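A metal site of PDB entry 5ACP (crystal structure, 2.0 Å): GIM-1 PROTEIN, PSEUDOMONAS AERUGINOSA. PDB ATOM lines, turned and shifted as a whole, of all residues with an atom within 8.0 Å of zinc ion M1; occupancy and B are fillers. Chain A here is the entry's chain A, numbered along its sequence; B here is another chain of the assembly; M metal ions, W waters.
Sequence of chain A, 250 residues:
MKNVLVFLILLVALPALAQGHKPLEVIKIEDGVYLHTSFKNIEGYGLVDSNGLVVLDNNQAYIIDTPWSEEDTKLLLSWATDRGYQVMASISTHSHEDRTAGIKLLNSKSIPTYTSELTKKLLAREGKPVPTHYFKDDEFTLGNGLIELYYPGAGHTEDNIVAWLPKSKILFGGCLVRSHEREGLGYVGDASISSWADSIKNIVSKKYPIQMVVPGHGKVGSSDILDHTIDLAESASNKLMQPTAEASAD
Water W1 binds zinc ion M1, at 1.9 Å.
NE2 of His 156 is bound to zinc ion M1 (2.0 Å).
Zinc ion M1 is bound by ND1 of His 96 (2.1 Å).
Zinc ion M1 is bound by NE2 of His 94 (2.3 Å).
Zinc ion M1 has four donor atoms within binding distance.
OCS 175 touches zinc ion M1.
Four residues have an atom within 4 Å of zinc ion M1: His 94, His 96, His 156 and OCS 175.
The nearest printed residue that does not touch zinc ion M1 is Asp 98 (4.04 Å).
N of His 156 sits at hydrogen-bond distance from OD1 of Asn 160, 3.0 Å away.
A ring nitrogen (NE2) of His 96 is in hydrogen-bond range of the side-chain carboxylate of Asp 190, at 2.7 Å.
OD3 of OCS 175 is in salt-bridge range of the guanidinium group (NE) of Arg 99, at 2.8 Å.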
ATOM      1  N   THR A  93       5.702   2.210  -7.958  1.00  0.00           N
ATOM      2  CA  THR A  93       5.663   0.991  -7.152  1.00  0.00           C
ATOM      3  C   THR A  93       6.895   0.097  -7.293  1.00  0.00           C
ATOM      4  O   THR A  93       7.009  -0.912  -6.596  1.00  0.00           O
ATOM      5  CB  THR A  93       4.389   0.166  -7.498  1.00  0.00           C
ATOM      6  OG1 THR A  93       4.356  -0.131  -8.893  1.00  0.00           O
ATOM      7  CG2 THR A  93       3.127   0.937  -7.116  1.00  0.00           C
ATOM      8  N   HIS A  94       7.807   0.445  -8.202  1.00  0.00           N
ATOM      9  CA  HIS A  94       9.194  -0.015  -8.158  1.00  0.00           C
ATOM     10  C   HIS A  94       9.968   0.771  -9.206  1.00  0.00           C
ATOM     11  O   HIS A  94       9.431   1.699  -9.788  1.00  0.00           O
ATOM     12  CB  HIS A  94       9.336  -1.532  -8.379  1.00  0.00           C
ATOM     13  CG  HIS A  94       8.894  -2.026  -9.719  1.00  0.00           C
ATOM     14  ND1 HIS A  94       7.581  -2.259 -10.026  1.00  0.00           N
ATOM     15  CD2 HIS A  94       9.620  -2.396 -10.805  1.00  0.00           C
ATOM     16  CE1 HIS A  94       7.503  -2.726 -11.270  1.00  0.00           C
ATOM     17  NE2 HIS A  94       8.717  -2.813 -11.762  1.00  0.00           N
ATOM     18  N   SER A  95      11.232   0.423  -9.428  1.00  0.00           N
ATOM     19  CA  SER A  95      12.131   1.329 -10.141  1.00  0.00           C
ATOM     20  C   SER A  95      12.070   1.218 -11.662  1.00  0.00           C
ATOM     21  O   SER A  95      12.606   2.078 -12.365  1.00  0.00           O
ATOM     22  CB  SER A  95      13.572   1.124  -9.678  1.00  0.00           C
ATOM     23  OG  SER A  95      14.133  -0.071 -10.208  1.00  0.00           O
ATOM     24  N   HIS A  96      11.424   0.175 -12.179  1.00  0.00           N
ATOM     25  CA  HIS A  96      11.449  -0.079 -13.621  1.00  0.00           C
ATOM     26  C   HIS A  96      10.770   1.028 -14.435  1.00  0.00           C
ATOM     27  O   HIS A  96       9.850   1.703 -13.968  1.00  0.00           O
ATOM     28  CB  HIS A  96      10.790  -1.415 -13.930  1.00  0.00           C
ATOM     29  CG  HIS A  96      11.652  -2.599 -13.637  1.00  0.00           C
ATOM     30  ND1 HIS A  96      11.175  -3.889 -13.692  1.00  0.00           N
ATOM     31  CD2 HIS A  96      12.958  -2.693 -13.294  1.00  0.00           C
ATOM     32  CE1 HIS A  96      12.159  -4.734 -13.387  1.00  0.00           C
ATOM     33  NE2 HIS A  96      13.243  -4.028 -13.146  1.00  0.00           N
ATOM     34  N   GLU A  97      11.251   1.172 -15.669  1.00  0.00           N
ATOM     35  CA  GLU A  97      10.814   2.212 -16.614  1.00  0.00           C
ATOM     36  C   GLU A  97       9.295   2.393 -16.701  1.00  0.00           C
ATOM     37  O   GLU A  97       8.810   3.530 -16.783  1.00  0.00           O
ATOM     38  CB  GLU A  97      11.359   1.876 -18.002  1.00  0.00           C
ATOM     39  CG  GLU A  97      11.220   2.989 -19.022  1.00  0.00           C
ATOM     40  CD  GLU A  97      12.190   4.129 -18.787  1.00  0.00           C
ATOM     41  OE1 GLU A  97      13.034   4.017 -17.884  1.00  0.00           O
ATOM     42  OE2 GLU A  97      12.115   5.132 -19.531  1.00  0.00           O
ATOM     43  N   ASP A  98       8.561   1.293 -16.708  1.00  0.00           N
ATOM     44  CA  ASP A  98       7.108   1.355 -16.894  1.00  0.00           C
ATOM     45  C   ASP A  98       6.398   1.920 -15.671  1.00  0.00           C
ATOM     46  O   ASP A  98       5.206   2.220 -15.722  1.00  0.00           O
ATOM     47  CB  ASP A  98       6.556  -0.021 -17.242  1.00  0.00           C
ATOM     48  CG  ASP A  98       6.841  -1.056 -16.179  1.00  0.00           C
ATOM     49  OD1 ASP A  98       8.025  -1.354 -15.921  1.00  0.00           O
ATOM     50  OD2 ASP A  98       5.868  -1.599 -15.611  1.00  0.00           O
ATOM     51  N   ARG A  99       7.141   2.064 -14.574  1.00  0.00           N
ATOM     52  CA  ARG A  99       6.616   2.652 -13.343  1.00  0.00           C
ATOM     53  C   ARG A  99       7.090   4.092 -13.126  1.00  0.00           C
ATOM     54  O   ARG A  99       6.442   4.863 -12.409  1.00  0.00           O
ATOM     55  CB  ARG A  99       7.030   1.811 -12.131  1.00  0.00           C
ATOM     56  CG  ARG A  99       6.759   0.316 -12.256  1.00  0.00           C
ATOM     57  CD  ARG A  99       5.280   0.024 -12.277  1.00  0.00           C
ATOM     58  NE  ARG A  99       4.825  -0.543 -13.542  1.00  0.00           N
ATOM     59  CZ  ARG A  99       3.550  -0.552 -13.934  1.00  0.00           C
ATOM     60  NH1 ARG A  99       2.609   0.002 -13.173  1.00  0.00           N
ATOM     61  NH2 ARG A  99       3.205  -1.098 -15.096  1.00  0.00           N
ATOM     62  N   HIS A 156       8.638  -9.756  -8.078  1.00  0.00           N
ATOM     63  CA  HIS A 156       8.992  -9.292  -9.419  1.00  0.00           C
ATOM     64  C   HIS A 156      10.319  -8.545  -9.369  1.00  0.00           C
ATOM     65  O   HIS A 156      11.166  -8.673 -10.265  1.00  0.00           O
ATOM     66  CB  HIS A 156       7.889  -8.407  -9.987  1.00  0.00           C
ATOM     67  CG  HIS A 156       8.278  -7.659 -11.216  1.00  0.00           C
ATOM     68  ND1 HIS A 156       8.356  -8.245 -12.466  1.00  0.00           N
ATOM     69  CD2 HIS A 156       8.600  -6.350 -11.410  1.00  0.00           C
ATOM     70  CE1 HIS A 156       8.709  -7.348 -13.354  1.00  0.00           C
ATOM     71  NE2 HIS A 156       8.872  -6.182 -12.738  1.00  0.00           N
ATOM     72  N   THR A 157      10.479  -7.743  -8.314  1.00  0.00           N
ATOM     73  CA  THR A 157      11.750  -7.079  -8.003  1.00  0.00           C
ATOM     74  C   THR A 157      12.007  -7.049  -6.490  1.00  0.00           C
ATOM     75  O   THR A 157      11.117  -7.383  -5.708  1.00  0.00           O
ATOM     76  CB  THR A 157      11.774  -5.631  -8.502  1.00  0.00           C
ATOM     77  OG1 THR A 157      10.614  -4.938  -8.020  1.00  0.00           O
ATOM     78  CG2 THR A 157      11.808  -5.580 -10.025  1.00  0.00           C
ATOM     79  N   ASP A 159      12.217  -4.464  -4.745  1.00  0.00           N
ATOM     80  CA  ASP A 159      11.656  -3.256  -4.180  1.00  0.00           C
ATOM     81  C   ASP A 159      10.153  -3.065  -4.411  1.00  0.00           C
ATOM     82  O   ASP A 159       9.606  -2.035  -4.011  1.00  0.00           O
ATOM     83  CB  ASP A 159      12.396  -2.040  -4.749  1.00  0.00           C
ATOM     84  CG  ASP A 159      12.249  -1.919  -6.255  1.00  0.00           C
ATOM     85  OD1 ASP A 159      12.338  -2.943  -6.951  1.00  0.00           O
ATOM     86  OD2 ASP A 159      12.046  -0.779  -6.738  1.00  0.00           O
ATOM     87  N   ASN A 160       9.488  -4.016  -5.059  1.00  0.00           N
ATOM     88  CA  ASN A 160       8.100  -3.779  -5.443  1.00  0.00           C
ATOM     89  C   ASN A 160       7.202  -3.577  -4.237  1.00  0.00           C
ATOM     90  O   ASN A 160       7.287  -4.293  -3.232  1.00  0.00           O
ATOM     91  CB  ASN A 160       7.533  -4.887  -6.346  1.00  0.00           C
ATOM     92  CG  ASN A 160       7.821  -6.299  -5.853  1.00  0.00           C
ATOM     93  OD1 ASN A 160       8.083  -7.204  -6.655  1.00  0.00           O
ATOM     94  ND2 ASN A 160       7.759  -6.508  -4.534  1.00  0.00           N
ATOM     95  N   GLY A 174       0.511  -3.847  -9.149  1.00  0.00           N
ATOM     96  CA  GLY A 174       1.630  -3.625 -10.046  1.00  0.00           C
ATOM     97  C   GLY A 174       2.139  -4.924 -10.643  1.00  0.00           C
ATOM     98  O   GLY A 174       1.368  -5.844 -10.898  1.00  0.00           O
ATOM     99  N   OCS A 175       3.451  -5.010 -10.862  1.00  0.00           N
ATOM    100  CA  OCS A 175       4.040  -6.182 -11.516  1.00  0.00           C
ATOM    101  CB  OCS A 175       5.300  -5.771 -12.269  1.00  0.00           C
ATOM    102  SG  OCS A 175       4.918  -4.598 -13.571  1.00  0.00           S
ATOM    103  C   OCS A 175       4.328  -7.332 -10.579  1.00  0.00           C
ATOM    104  O   OCS A 175       4.786  -8.394 -10.998  1.00  0.00           O
ATOM    105  OD1 OCS A 175       3.668  -4.965 -14.119  1.00  0.00           O
ATOM    106  OD2 OCS A 175       5.902  -4.641 -14.595  1.00  0.00           O
ATOM    107  OD3 OCS A 175       4.808  -3.294 -13.021  1.00  0.00           O
ATOM    108  N   LEU A 176       4.043  -7.136  -9.299  1.00  0.00           N
ATOM    109  CA  LEU A 176       4.111  -8.213  -8.323  1.00  0.00           C
ATOM    110  C   LEU A 176       2.998  -9.221  -8.578  1.00  0.00           C
ATOM    111  O   LEU A 176       3.117 -10.387  -8.182  1.00  0.00           O
ATOM    112  CB  LEU A 176       4.014  -7.642  -6.908  1.00  0.00           C
ATOM    113  CG  LEU A 176       4.122  -8.622  -5.743  1.00  0.00           C
ATOM    114  CD1 LEU A 176       5.389  -9.460  -5.816  1.00  0.00           C
ATOM    115  CD2 LEU A 176       4.043  -7.871  -4.425  1.00  0.00           C
ATOM    116  N   TYR A 187       9.079 -10.876 -17.069  1.00  0.00           N
ATOM    117  CA  TYR A 187      10.491 -10.543 -16.878  1.00  0.00           C
ATOM    118  C   TYR A 187      10.954 -10.892 -15.467  1.00  0.00           C
ATOM    119  O   TYR A 187      10.545 -10.252 -14.493  1.00  0.00           O
ATOM    120  CB  TYR A 187      10.732  -9.050 -17.137  1.00  0.00           C
ATOM    121  CG  TYR A 187      12.171  -8.645 -17.001  1.00  0.00           C
ATOM    122  CD1 TYR A 187      13.087  -8.936 -18.006  1.00  0.00           C
ATOM    123  CD2 TYR A 187      12.622  -7.978 -15.882  1.00  0.00           C
ATOM    124  CE1 TYR A 187      14.413  -8.562 -17.892  1.00  0.00           C
ATOM    125  CE2 TYR A 187      13.942  -7.595 -15.749  1.00  0.00           C
ATOM    126  CZ  TYR A 187      14.837  -7.898 -16.755  1.00  0.00           C
ATOM    127  OH  TYR A 187      16.157  -7.524 -16.633  1.00  0.00           O
ATOM    128  N   ASP A 190      15.217  -9.336 -12.788  1.00  0.00           N
ATOM    129  CA  ASP A 190      15.436  -8.661 -11.507  1.00  0.00           C
ATOM    130  C   ASP A 190      14.638  -9.309 -10.382  1.00  0.00           C
ATOM    131  O   ASP A 190      14.495  -8.736  -9.300  1.00  0.00           O
ATOM    132  CB  ASP A 190      15.067  -7.179 -11.627  1.00  0.00           C
ATOM    133  CG  ASP A 190      15.970  -6.427 -12.572  1.00  0.00           C
ATOM    134  OD1 ASP A 190      17.192  -6.656 -12.538  1.00  0.00           O
ATOM    135  OD2 ASP A 190      15.456  -5.601 -13.362  1.00  0.00           O
ATOM    136  N   HIS A 217       0.367  -4.960 -15.855  1.00  0.00           N
ATOM    137  CA  HIS A 217       0.042  -5.253 -17.255  1.00  0.00           C
ATOM    138  C   HIS A 217      -1.124  -6.221 -17.319  1.00  0.00           C
ATOM    139  O   HIS A 217      -1.239  -7.114 -16.483  1.00  0.00           O
ATOM    140  CB  HIS A 217       1.240  -5.810 -17.998  1.00  0.00           C
ATOM    141  CG  HIS A 217       2.501  -5.050 -17.765  1.00  0.00           C
ATOM    142  ND1 HIS A 217       2.778  -3.862 -18.422  1.00  0.00           N
ATOM    143  CD2 HIS A 217       3.537  -5.278 -16.941  1.00  0.00           C
ATOM    144  CE1 HIS A 217       3.942  -3.396 -17.998  1.00  0.00           C
ATOM    145  NE2 HIS A 217       4.432  -4.240 -17.105  1.00  0.00           N
ATOM    146  N   ILE B  42      13.478  -5.407 -22.533  1.00  0.00           N
ATOM    147  CA  ILE B  42      12.399  -4.422 -22.605  1.00  0.00           C
ATOM    148  C   ILE B  42      11.758  -4.301 -21.227  1.00  0.00           C
ATOM    149  O   ILE B  42      10.952  -5.148 -20.834  1.00  0.00           O
ATOM    150  CB  ILE B  42      11.340  -4.808 -23.647  1.00  0.00           C
ATOM    151  CG1 ILE B  42      11.973  -4.897 -25.043  1.00  0.00           C
ATOM    152  CG2 ILE B  42      10.200  -3.791 -23.652  1.00  0.00           C
ATOM    153  N   GLU B  43      12.121  -3.248 -20.509  1.00  0.00           N
ATOM    154  CA  GLU B  43      11.619  -3.039 -19.151  1.00  0.00           C
ATOM    155  C   GLU B  43      10.113  -2.879 -19.149  1.00  0.00           C
ATOM    156  O   GLU B  43       9.571  -1.929 -19.722  1.00  0.00           O
ATOM    157  CB  GLU B  43      12.274  -1.806 -18.514  1.00  0.00           C
ATOM    158  CG  GLU B  43      13.794  -1.897 -18.379  1.00  0.00           C
ATOM    159  CD  GLU B  43      14.238  -2.828 -17.266  1.00  0.00           C
ATOM    160  OE1 GLU B  43      13.379  -3.577 -16.730  1.00  0.00           O
ATOM    161  OE2 GLU B  43      15.437  -2.814 -16.921  1.00  0.00           O
ATOM    162  N   GLY B  44       9.425  -3.828 -18.515  1.00  0.00           N
ATOM    163  CA  GLY B  44       7.979  -3.789 -18.391  1.00  0.00           C
ATOM    164  C   GLY B  44       7.283  -4.902 -19.139  1.00  0.00           C
ATOM    165  O   GLY B  44       6.065  -4.877 -19.307  1.00  0.00           O
ATOM    166  N   TYR B  45       8.028  -5.891 -19.615  1.00  0.00           N
ATOM    167  CA  TYR B  45       7.406  -7.004 -20.329  1.00  0.00           C
ATOM    168  C   TYR B  45       8.292  -8.260 -20.385  1.00  0.00           C
ATOM    169  O   TYR B  45       7.799  -9.366 -20.135  1.00  0.00           O
ATOM    170  CB  TYR B  45       7.040  -6.561 -21.752  1.00  0.00           C
ATOM    171  CG  TYR B  45       7.446  -7.539 -22.818  1.00  0.00           C
ATOM    172  CD1 TYR B  45       6.589  -8.557 -23.231  1.00  0.00           C
ATOM    173  CD2 TYR B  45       8.688  -7.447 -23.424  1.00  0.00           C
ATOM    174  CE1 TYR B  45       6.966  -9.455 -24.209  1.00  0.00           C
ATOM    175  CE2 TYR B  45       9.069  -8.337 -24.400  1.00  0.00           C
ATOM    176  CZ  TYR B  45       8.203  -9.332 -24.796  1.00  0.00           C
ATOM    177  OH  TYR B  45       8.584 -10.221 -25.771  1.00  0.00           O
HETATM  178 ZN    ZN M   1       9.172  -4.310 -13.425  1.00  0.00          ZN
HETATM  179 ZN    ZN M   2       5.848  -3.403 -15.835  1.00  0.00          ZN
HETATM  180  O   HOH W   1       8.098  -3.798 -14.901  1.00  0.00           O
